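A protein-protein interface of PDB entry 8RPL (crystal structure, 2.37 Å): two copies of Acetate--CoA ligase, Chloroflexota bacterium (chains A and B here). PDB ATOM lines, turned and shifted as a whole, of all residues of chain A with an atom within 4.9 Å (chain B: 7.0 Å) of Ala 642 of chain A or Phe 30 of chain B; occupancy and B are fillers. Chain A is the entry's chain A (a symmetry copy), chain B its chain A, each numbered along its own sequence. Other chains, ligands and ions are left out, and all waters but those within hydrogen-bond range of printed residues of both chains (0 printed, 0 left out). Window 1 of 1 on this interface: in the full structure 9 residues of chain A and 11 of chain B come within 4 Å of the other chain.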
ATOM      1  N   ARG A 638      30.874 -22.669  -1.542  1.00  0.00           N
ATOM      2  CA  ARG A 638      29.798 -23.137  -2.407  1.00  0.00           C
ATOM      3  C   ARG A 638      28.902 -24.128  -1.658  1.00  0.00           C
ATOM      4  O   ARG A 638      27.685 -24.108  -1.843  1.00  0.00           O
ATOM      5  CB  ARG A 638      30.316 -23.766  -3.709  1.00  0.00           C
ATOM      6  CG  ARG A 638      31.157 -22.778  -4.497  1.00  0.00           C
ATOM      7  CD  ARG A 638      30.791 -22.617  -5.968  1.00  0.00           C
ATOM      8  NE  ARG A 638      31.577 -21.452  -6.394  1.00  0.00           N
ATOM      9  CZ  ARG A 638      32.791 -21.521  -6.938  1.00  0.00           C
ATOM     10  NH1 ARG A 638      33.195 -22.642  -7.517  1.00  0.00           N
ATOM     11  NH2 ARG A 638      33.576 -20.455  -6.939  1.00  0.00           N
ATOM     12  N   VAL A 639      29.510 -24.975  -0.813  1.00  0.00           N
ATOM     13  CA  VAL A 639      28.756 -25.940  -0.041  1.00  0.00           C
ATOM     14  C   VAL A 639      27.934 -25.227   1.030  1.00  0.00           C
ATOM     15  O   VAL A 639      26.795 -25.614   1.273  1.00  0.00           O
ATOM     16  CB  VAL A 639      29.674 -27.035   0.516  1.00  0.00           C
ATOM     17  CG1 VAL A 639      28.927 -28.071   1.354  1.00  0.00           C
ATOM     18  CG2 VAL A 639      30.371 -27.739  -0.639  1.00  0.00           C
ATOM     19  N   VAL A 640      28.464 -24.142   1.591  1.00  0.00           N
ATOM     20  CA  VAL A 640      27.764 -23.424   2.644  1.00  0.00           C
ATOM     21  C   VAL A 640      26.480 -22.861   2.053  1.00  0.00           C
ATOM     22  O   VAL A 640      25.415 -23.001   2.650  1.00  0.00           O
ATOM     23  CB  VAL A 640      28.566 -22.299   3.337  1.00  0.00           C
ATOM     24  CG1 VAL A 640      27.679 -21.467   4.254  1.00  0.00           C
ATOM     25  CG2 VAL A 640      29.740 -22.853   4.135  1.00  0.00           C
ATOM     26  N   ARG A 641      26.630 -22.230   0.887  1.00  0.00           N
ATOM     27  CA  ARG A 641      25.544 -21.566   0.180  1.00  0.00           C
ATOM     28  C   ARG A 641      24.527 -22.593  -0.310  1.00  0.00           C
ATOM     29  O   ARG A 641      23.328 -22.438  -0.089  1.00  0.00           O
ATOM     30  CB  ARG A 641      26.157 -20.771  -0.970  1.00  0.00           C
ATOM     31  CG  ARG A 641      25.184 -19.745  -1.521  1.00  0.00           C
ATOM     32  CD  ARG A 641      25.644 -19.071  -2.801  1.00  0.00           C
ATOM     33  NE  ARG A 641      24.739 -17.925  -2.988  1.00  0.00           N
ATOM     34  CZ  ARG A 641      23.617 -17.958  -3.733  1.00  0.00           C
ATOM     35  NH1 ARG A 641      23.184 -19.086  -4.285  1.00  0.00           N
ATOM     36  NH2 ARG A 641      22.883 -16.875  -3.892  1.00  0.00           N
ATOM     37  N   ALA A 642      25.032 -23.692  -0.882  1.00  0.00           N
ATOM     38  CA  ALA A 642      24.179 -24.768  -1.360  1.00  0.00           C
ATOM     39  C   ALA A 642      23.355 -25.357  -0.216  1.00  0.00           C
ATOM     40  O   ALA A 642      22.188 -25.672  -0.451  1.00  0.00           O
ATOM     41  CB  ALA A 642      24.999 -25.840  -2.055  1.00  0.00           C
ATOM     42  N   ARG A 643      23.960 -25.543   0.979  1.00  0.00           N
ATOM     43  CA  ARG A 643      23.215 -26.029   2.140  1.00  0.00           C
ATOM     44  C   ARG A 643      22.083 -25.045   2.462  1.00  0.00           C
ATOM     45  O   ARG A 643      20.977 -25.463   2.794  1.00  0.00           O
ATOM     46  CB  ARG A 643      23.989 -26.223   3.450  1.00  0.00           C
ATOM     47  CG  ARG A 643      25.041 -27.314   3.418  1.00  0.00           C
ATOM     48  CD  ARG A 643      25.575 -27.649   4.819  1.00  0.00           C
ATOM     49  NE  ARG A 643      26.463 -28.818   4.718  1.00  0.00           N
ATOM     50  CZ  ARG A 643      27.761 -28.881   5.038  1.00  0.00           C
ATOM     51  NH1 ARG A 643      28.326 -27.889   5.708  1.00  0.00           N
ATOM     52  NH2 ARG A 643      28.484 -29.948   4.705  1.00  0.00           N
ATOM     53  N   GLU A 644      22.361 -23.745   2.384  1.00  0.00           N
ATOM     54  CA  GLU A 644      21.328 -22.771   2.676  1.00  0.00           C
ATOM     55  C   GLU A 644      20.293 -22.693   1.560  1.00  0.00           C
ATOM     56  O   GLU A 644      19.123 -22.777   1.857  1.00  0.00           O
ATOM     57  CB  GLU A 644      21.865 -21.352   2.843  1.00  0.00           C
ATOM     58  CG  GLU A 644      22.242 -21.029   4.282  1.00  0.00           C
ATOM     59  CD  GLU A 644      21.154 -20.386   5.134  1.00  0.00           C
ATOM     60  OE1 GLU A 644      20.730 -19.217   4.875  1.00  0.00           O
ATOM     61  OE2 GLU A 644      20.789 -21.075   6.108  1.00  0.00           O
ATOM     62  N   LEU A 645      20.729 -22.493   0.307  1.00  0.00           N
ATOM     63  CA  LEU A 645      19.856 -22.054  -0.777  1.00  0.00           C
ATOM     64  C   LEU A 645      19.619 -23.128  -1.833  1.00  0.00           C
ATOM     65  O   LEU A 645      18.739 -22.948  -2.659  1.00  0.00           O
ATOM     66  CB  LEU A 645      20.485 -20.826  -1.424  1.00  0.00           C
ATOM     67  CG  LEU A 645      20.501 -19.579  -0.534  1.00  0.00           C
ATOM     68  CD1 LEU A 645      21.297 -18.470  -1.174  1.00  0.00           C
ATOM     69  CD2 LEU A 645      19.090 -19.098  -0.197  1.00  0.00           C
ATOM     70  N   GLY A 646      20.393 -24.222  -1.800  1.00  0.00           N
ATOM     71  CA  GLY A 646      20.427 -25.197  -2.875  1.00  0.00           C
ATOM     72  C   GLY A 646      21.364 -24.744  -3.992  1.00  0.00           C
ATOM     73  O   GLY A 646      21.645 -23.562  -4.092  1.00  0.00           O
ATOM     74  N   GLU A 647      21.844 -25.696  -4.807  1.00  0.00           N
ATOM     75  CA  GLU A 647      22.677 -25.422  -5.976  1.00  0.00           C
ATOM     76  C   GLU A 647      21.919 -25.840  -7.238  1.00  0.00           C
ATOM     77  O   GLU A 647      21.457 -26.986  -7.304  1.00  0.00           O
ATOM     78  CB  GLU A 647      23.977 -26.226  -5.879  1.00  0.00           C
ATOM     79  CG  GLU A 647      25.073 -25.745  -6.828  1.00  0.00           C
ATOM     80  CD  GLU A 647      26.441 -25.651  -6.154  1.00  0.00           C
ATOM     81  OE1 GLU A 647      26.953 -26.734  -5.777  1.00  0.00           O
ATOM     82  OE2 GLU A 647      26.969 -24.518  -5.955  1.00  0.00           O
ATOM     83  N   ILE B  25      12.873 -24.019  -7.933  1.00  0.00           N
ATOM     84  CA  ILE B  25      13.240 -24.568  -6.632  1.00  0.00           C
ATOM     85  C   ILE B  25      13.425 -26.094  -6.665  1.00  0.00           C
ATOM     86  O   ILE B  25      14.357 -26.583  -6.033  1.00  0.00           O
ATOM     87  CB  ILE B  25      12.235 -24.111  -5.554  1.00  0.00           C
ATOM     88  CG1 ILE B  25      12.557 -24.739  -4.177  1.00  0.00           C
ATOM     89  CG2 ILE B  25      10.781 -24.346  -5.985  1.00  0.00           C
ATOM     90  CD1 ILE B  25      13.973 -24.447  -3.697  1.00  0.00           C
ATOM     91  N   GLU B  26      12.577 -26.837  -7.407  1.00  0.00           N
ATOM     92  CA  GLU B  26      12.647 -28.291  -7.534  1.00  0.00           C
ATOM     93  C   GLU B  26      13.939 -28.771  -8.196  1.00  0.00           C
ATOM     94  O   GLU B  26      14.280 -29.935  -8.051  1.00  0.00           O
ATOM     95  CB  GLU B  26      11.593 -28.896  -8.469  1.00  0.00           C
ATOM     96  CG  GLU B  26      10.156 -28.788  -7.980  1.00  0.00           C
ATOM     97  CD  GLU B  26       9.243 -28.039  -8.945  1.00  0.00           C
ATOM     98  OE1 GLU B  26       9.360 -26.783  -9.030  1.00  0.00           O
ATOM     99  OE2 GLU B  26       8.420 -28.707  -9.616  1.00  0.00           O
ATOM    100  N   GLU B  27      14.602 -27.927  -8.992  1.00  0.00           N
ATOM    101  CA  GLU B  27      15.814 -28.325  -9.694  1.00  0.00           C
ATOM    102  C   GLU B  27      17.081 -27.990  -8.894  1.00  0.00           C
ATOM    103  O   GLU B  27      18.177 -28.050  -9.433  1.00  0.00           O
ATOM    104  CB  GLU B  27      15.849 -27.686 -11.089  1.00  0.00           C
ATOM    105  CG  GLU B  27      15.028 -28.437 -12.137  1.00  0.00           C
ATOM    106  CD  GLU B  27      15.145 -29.963 -12.097  1.00  0.00           C
ATOM    107  OE1 GLU B  27      16.282 -30.507 -12.021  1.00  0.00           O
ATOM    108  OE2 GLU B  27      14.078 -30.623 -12.131  1.00  0.00           O
ATOM    109  N   ARG B  28      16.946 -27.630  -7.614  1.00  0.00           N
ATOM    110  CA  ARG B  28      18.097 -27.287  -6.801  1.00  0.00           C
ATOM    111  C   ARG B  28      18.545 -28.523  -6.032  1.00  0.00           C
ATOM    112  O   ARG B  28      17.737 -29.349  -5.606  1.00  0.00           O
ATOM    113  CB  ARG B  28      17.779 -26.085  -5.900  1.00  0.00           C
ATOM    114  CG  ARG B  28      17.666 -24.787  -6.690  1.00  0.00           C
ATOM    115  CD  ARG B  28      17.024 -23.623  -5.923  1.00  0.00           C
ATOM    116  NE  ARG B  28      18.110 -22.802  -5.385  1.00  0.00           N
ATOM    117  CZ  ARG B  28      18.796 -21.921  -6.094  1.00  0.00           C
ATOM    118  NH1 ARG B  28      18.209 -21.222  -7.044  1.00  0.00           N
ATOM    119  NH2 ARG B  28      20.057 -21.690  -5.795  1.00  0.00           N
ATOM    120  N   LEU B  29      19.856 -28.635  -5.854  1.00  0.00           N
ATOM    121  CA  LEU B  29      20.447 -29.746  -5.143  1.00  0.00           C
ATOM    122  C   LEU B  29      20.954 -29.263  -3.790  1.00  0.00           C
ATOM    123  O   LEU B  29      21.657 -28.254  -3.706  1.00  0.00           O
ATOM    124  CB  LEU B  29      21.572 -30.191  -6.061  1.00  0.00           C
ATOM    125  CG  LEU B  29      21.897 -31.678  -6.038  1.00  0.00           C
ATOM    126  CD1 LEU B  29      20.693 -32.421  -6.556  1.00  0.00           C
ATOM    127  CD2 LEU B  29      23.136 -31.965  -6.861  1.00  0.00           C
ATOM    128  N   PHE B  30      20.575 -29.972  -2.727  1.00  0.00           N
ATOM    129  CA  PHE B  30      20.951 -29.573  -1.381  1.00  0.00           C
ATOM    130  C   PHE B  30      21.903 -30.607  -0.809  1.00  0.00           C
ATOM    131  O   PHE B  30      21.493 -31.723  -0.567  1.00  0.00           O
ATOM    132  CB  PHE B  30      19.733 -29.496  -0.458  1.00  0.00           C
ATOM    133  CG  PHE B  30      18.816 -28.343  -0.816  1.00  0.00           C
ATOM    134  CD1 PHE B  30      17.913 -28.458  -1.858  1.00  0.00           C
ATOM    135  CD2 PHE B  30      18.882 -27.148  -0.123  1.00  0.00           C
ATOM    136  CE1 PHE B  30      17.070 -27.418  -2.173  1.00  0.00           C
ATOM    137  CE2 PHE B  30      18.056 -26.100  -0.466  1.00  0.00           C
ATOM    138  CZ  PHE B  30      17.158 -26.237  -1.492  1.00  0.00           C
ATOM    139  N   PRO B  31      23.194 -30.302  -0.590  1.00  0.00           N
ATOM    140  CA  PRO B  31      24.105 -31.315  -0.082  1.00  0.00           C
ATOM    141  C   PRO B  31      23.868 -31.685   1.381  1.00  0.00           C
ATOM    142  O   PRO B  31      23.301 -30.905   2.160  1.00  0.00           O
ATOM    143  CB  PRO B  31      25.475 -30.714  -0.314  1.00  0.00           C
ATOM    144  CG  PRO B  31      25.238 -29.225  -0.289  1.00  0.00           C
ATOM    145  CD  PRO B  31      23.841 -29.008  -0.835  1.00  0.00           C
ATOM    146  N   PRO B  32      24.145 -32.937   1.815  1.00  0.00           N
ATOM    147  CA  PRO B  32      23.866 -33.317   3.204  1.00  0.00           C
ATOM    148  C   PRO B  32      24.612 -32.444   4.226  1.00  0.00           C
ATOM    149  O   PRO B  32      25.638 -31.850   3.895  1.00  0.00           O
ATOM    150  CB  PRO B  32      24.278 -34.805   3.274  1.00  0.00           C
ATOM    151  CG  PRO B  32      25.040 -35.103   1.996  1.00  0.00           C
ATOM    152  CD  PRO B  32      24.723 -34.021   1.001  1.00  0.00           C
ATOM    153  N   PRO B  33      24.128 -32.320   5.492  1.00  0.00           N
ATOM    154  CA  PRO B  33      24.836 -31.528   6.517  1.00  0.00           C
ATOM    155  C   PRO B  33      26.238 -32.009   6.930  1.00  0.00           C
ATOM    156  O   PRO B  33      26.832 -32.862   6.272  1.00  0.00           O
ATOM    157  CB  PRO B  33      23.828 -31.534   7.708  1.00  0.00           C
ATOM    158  CG  PRO B  33      22.975 -32.760   7.489  1.00  0.00           C
ATOM    159  CD  PRO B  33      22.858 -32.896   5.977  1.00  0.00           C
ATOM    160  N   TRP B 422       8.127 -28.641   1.411  1.00  0.00           N
ATOM    161  CA  TRP B 422       9.438 -29.226   1.633  1.00  0.00           C
ATOM    162  C   TRP B 422      10.353 -28.171   2.245  1.00  0.00           C
ATOM    163  O   TRP B 422      10.977 -28.412   3.266  1.00  0.00           O
ATOM    164  CB  TRP B 422       9.971 -29.749   0.293  1.00  0.00           C
ATOM    165  CG  TRP B 422      11.262 -30.519   0.339  1.00  0.00           C
ATOM    166  CD1 TRP B 422      11.391 -31.872   0.330  1.00  0.00           C
ATOM    167  CD2 TRP B 422      12.607 -29.990   0.370  1.00  0.00           C
ATOM    168  NE1 TRP B 422      12.719 -32.221   0.357  1.00  0.00           N
ATOM    169  CE2 TRP B 422      13.485 -31.090   0.392  1.00  0.00           C
ATOM    170  CE3 TRP B 422      13.151 -28.708   0.388  1.00  0.00           C
ATOM    171  CZ2 TRP B 422      14.867 -30.947   0.437  1.00  0.00           C
ATOM    172  CZ3 TRP B 422      14.526 -28.564   0.422  1.00  0.00           C
ATOM    173  CH2 TRP B 422      15.369 -29.665   0.449  1.00  0.00           C
ATOM    174  N   MET B 423      10.347 -26.971   1.665  1.00  0.00           N
ATOM    175  CA  MET B 423      11.107 -25.834   2.174  1.00  0.00           C
ATOM    176  C   MET B 423      10.688 -25.472   3.600  1.00  0.00           C
ATOM    177  O   MET B 423      11.549 -25.249   4.447  1.00  0.00           O
ATOM    178  CB  MET B 423      10.974 -24.616   1.250  1.00  0.00           C
ATOM    179  CG  MET B 423      11.748 -24.750  -0.086  1.00  0.00           C
ATOM    180  SD  MET B 423      13.535 -25.079  -0.030  1.00  0.00           S
ATOM    181  CE  MET B 423      14.209 -24.013   1.263  1.00  0.00           C
ATOM    182  N   ARG B 426      12.033 -28.130   5.942  1.00  0.00           N
ATOM    183  CA  ARG B 426      13.467 -28.065   6.086  1.00  0.00           C
ATOM    184  C   ARG B 426      13.859 -26.819   6.878  1.00  0.00           C
ATOM    185  O   ARG B 426      14.796 -26.866   7.666  1.00  0.00           O
ATOM    186  CB  ARG B 426      14.120 -28.050   4.700  1.00  0.00           C
ATOM    187  CG  ARG B 426      15.633 -27.948   4.825  1.00  0.00           C
ATOM    188  CD  ARG B 426      16.330 -28.393   3.600  1.00  0.00           C
ATOM    189  NE  ARG B 426      17.641 -27.749   3.494  1.00  0.00           N
ATOM    190  CZ  ARG B 426      18.775 -28.436   3.536  1.00  0.00           C
ATOM    191  NH1 ARG B 426      18.803 -29.723   3.865  1.00  0.00           N
ATOM    192  NH2 ARG B 426      19.886 -27.811   3.261  1.00  0.00           N
ATOM    193  N   ASN B 432      17.221 -25.412   8.169  1.00  0.00           N
ATOM    194  CA  ASN B 432      17.902 -25.289   6.880  1.00  0.00           C
ATOM    195  C   ASN B 432      19.137 -26.185   6.762  1.00  0.00           C
ATOM    196  O   ASN B 432      20.075 -25.845   6.048  1.00  0.00           O
ATOM    197  CB  ASN B 432      18.342 -23.859   6.568  1.00  0.00           C
ATOM    198  CG  ASN B 432      17.226 -22.990   6.038  1.00  0.00           C
ATOM    199  OD1 ASN B 432      16.378 -23.432   5.257  1.00  0.00           O
ATOM    200  ND2 ASN B 432      17.206 -21.736   6.455  1.00  0.00           N
ATOM    201  N   LEU B 456      22.994 -38.915   0.108  1.00  0.00           N
ATOM    202  CA  LEU B 456      22.603 -38.396  -1.193  1.00  0.00           C
ATOM    203  C   LEU B 456      22.225 -36.925  -1.110  1.00  0.00           C
ATOM    204  O   LEU B 456      21.364 -36.527  -0.341  1.00  0.00           O
ATOM    205  CB  LEU B 456      21.430 -39.166  -1.786  1.00  0.00           C
ATOM    206  CG  LEU B 456      21.781 -40.453  -2.532  1.00  0.00           C
ATOM    207  CD1 LEU B 456      20.468 -41.002  -3.033  1.00  0.00           C
ATOM    208  CD2 LEU B 456      22.756 -40.266  -3.666  1.00  0.00           C
ATOM    209  N   PRO B 457      22.744 -36.094  -2.025  1.00  0.00           N
ATOM    210  CA  PRO B 457      22.210 -34.744  -2.198  1.00  0.00           C
ATOM    211  C   PRO B 457      20.737 -34.811  -2.600  1.00  0.00           C
ATOM    212  O   PRO B 457      20.319 -35.743  -3.281  1.00  0.00           O
ATOM    213  CB  PRO B 457      23.110 -34.078  -3.251  1.00  0.00           C
ATOM    214  CG  PRO B 457      23.919 -35.219  -3.863  1.00  0.00           C
ATOM    215  CD  PRO B 457      23.824 -36.429  -2.955  1.00  0.00           C
ATOM    216  N   LEU B 458      19.949 -33.847  -2.109  1.00  0.00           N
ATOM    217  CA  LEU B 458      18.498 -33.909  -2.171  1.00  0.00           C
ATOM    218  C   LEU B 458      17.980 -32.899  -3.187  1.00  0.00           C
ATOM    219  O   LEU B 458      18.558 -31.822  -3.323  1.00  0.00           O
ATOM    220  CB  LEU B 458      17.947 -33.605  -0.788  1.00  0.00           C
ATOM    221  CG  LEU B 458      18.431 -34.513   0.342  1.00  0.00           C
ATOM    222  CD1 LEU B 458      17.776 -34.126   1.637  1.00  0.00           C
ATOM    223  CD2 LEU B 458      18.104 -35.953   0.040  1.00  0.00           C
ATOM    224  N   LYS B 459      16.874 -33.275  -3.852  1.00  0.00           N
ATOM    225  CA  LYS B 459      16.056 -32.384  -4.666  1.00  0.00           C
ATOM    226  C   LYS B 459      14.628 -32.302  -4.120  1.00  0.00           C
ATOM    227  O   LYS B 459      13.943 -33.315  -3.994  1.00  0.00           O
ATOM    228  CB  LYS B 459      15.956 -32.838  -6.121  1.00  0.00           C
ATOM    229  CG  LYS B 459      17.188 -32.615  -6.984  1.00  0.00           C
ATOM    230  CD  LYS B 459      16.894 -32.953  -8.443  1.00  0.00           C
ATOM    231  CE  LYS B 459      18.165 -32.939  -9.238  1.00  0.00           C
ATOM    232  NZ  LYS B 459      18.071 -33.564 -10.559  1.00  0.00           N
ATOM    233  N   PRO B 460      14.092 -31.089  -3.852  1.00  0.00           N
ATOM    234  CA  PRO B 460      12.742 -30.946  -3.306  1.00  0.00           C
ATOM    235  C   PRO B 460      11.688 -31.667  -4.140  1.00  0.00           C
ATOM    236  O   PRO B 460      11.563 -31.400  -5.315  1.00  0.00           O
ATOM    237  CB  PRO B 460      12.508 -29.441  -3.320  1.00  0.00           C
ATOM    238  CG  PRO B 460      13.887 -28.852  -3.303  1.00  0.00           C
ATOM    239  CD  PRO B 460      14.735 -29.793  -4.104  1.00  0.00           C
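Ala 642 of chain A touches just these residues of chain B: Phe 30 and Pro 31. Of chain A, only Ala 642, Arg 643, Leu 645 and Gly 646 come within 4 Å of Phe 30 of chain B. Printed residues of chain A within 4 Å of Pro 31 of chain B: Ala 642 (3.6 Å) and Arg 643 (3.9 Å). Of the printed residues of chain A, Asn 432 of chain B touches Arg 643 (3.4 Å) and Glu 644 (3.7 Å). Of the printed residues of chain A, Arg 426 of chain B touches Arg 643 (2.6 Å). Of the printed residues of chain A, Arg 28 of chain B touches Leu 645, Gly 646 and Glu 647. Printed residues of chain A within 4 Å of Pro 33 of chain B: Arg 643. Leu 458 of chain B touches none of the printed residues of chain A. The nearest printed residue of chain A that does not touch Asn 432 of chain B is Leu 645 of chain A (6.7 Å).
No position is printed for both chains.
Printed residues of chain A that touch a printed residue of chain B: Ala 642, Arg 643, Glu 644, Leu 645, Gly 646 and Glu 647. Along chain A the printed residues that touch a printed residue of chain B span positions 642 to 647. Printed residues of chain B that touch a printed residue of chain A: Arg 28, Leu 29, Phe 30, Pro 31, Pro 32, Pro 33, Arg 426 and Asn 432. Hydrophobic or aromatic side chains of chain B that line the printed part of chain A: Leu 29, Phe 30 and Pro 31. Along chain B the printed residues that touch a printed residue of chain A span positions 28 to 432. Among the printed residues, no Asp or Glu carboxylate lies within 4 Å of a Lys or Arg side-chain nitrogen of the other chain.
N of Phe 30 of chain B sits at hydrogen-bond distance from O of Leu 458 of chain B (2.8 Å). The backbone carbonyl oxygen (O) of Arg 426 of chain B sits at hydrogen-bond distance from the backbone NH (N) of Asn 432 of chain B (2.9 Å).
NE of Arg 28 of chain B lies within hydrogen-bond range of O of Leu 645 of chain A, 2.8 Å away. O of Gly 646 of chain A is in hydrogen-bond range of NH2 of Arg 28 of chain B, at 3.0 Å. The backbone NH of Leu 29 of chain B is in hydrogen-bond range of the backbone carbonyl oxygen of Glu 647 of chain A, 2.7 Å away. O of Pro 32 of chain B sits at hydrogen-bond distance from NE of Arg 643 of chain A (3.2 Å). The guanidinium group (NH2) of Arg 426 of chain B lies within hydrogen-bond range of the backbone carbonyl oxygen (O) of Arg 643 of chain A. The backbone carbonyl oxygen of Asn 432 of chain B sits close to the backbone carbonyl oxygen of Arg 643 of chain A, 3.4 Å away.
CD2 of Phe 30 of chain B touches O of Ala 642 of chain A, 3.6 Å away. Ala 642 of chain A touches Pro 31 of chain B. CD2 of Phe 30 of chain B touches O of Arg 643 of chain A, at 3.97 Å. CD of Pro 31 of chain B touches N of Arg 643 of chain A, 3.9 Å away. NE of Arg 643 of chain A touches CA of Pro 33 of chain B, 3.6 Å away. Glu 644 of chain A touches Asn 432 of chain B (OE2 to ND2, 3.7 Å). Leu 645 of chain A touches Phe 30 of chain B. Gly 646 of chain A touches Leu 29 of chain B (CA to O, 3.4 Å). Phe 30 of chain B touches Gly 646 of chain A (CE2 to N, 3.3 Å). Glu 647 of chain A touches Arg 28 of chain B (O to CA, 3.4 Å).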
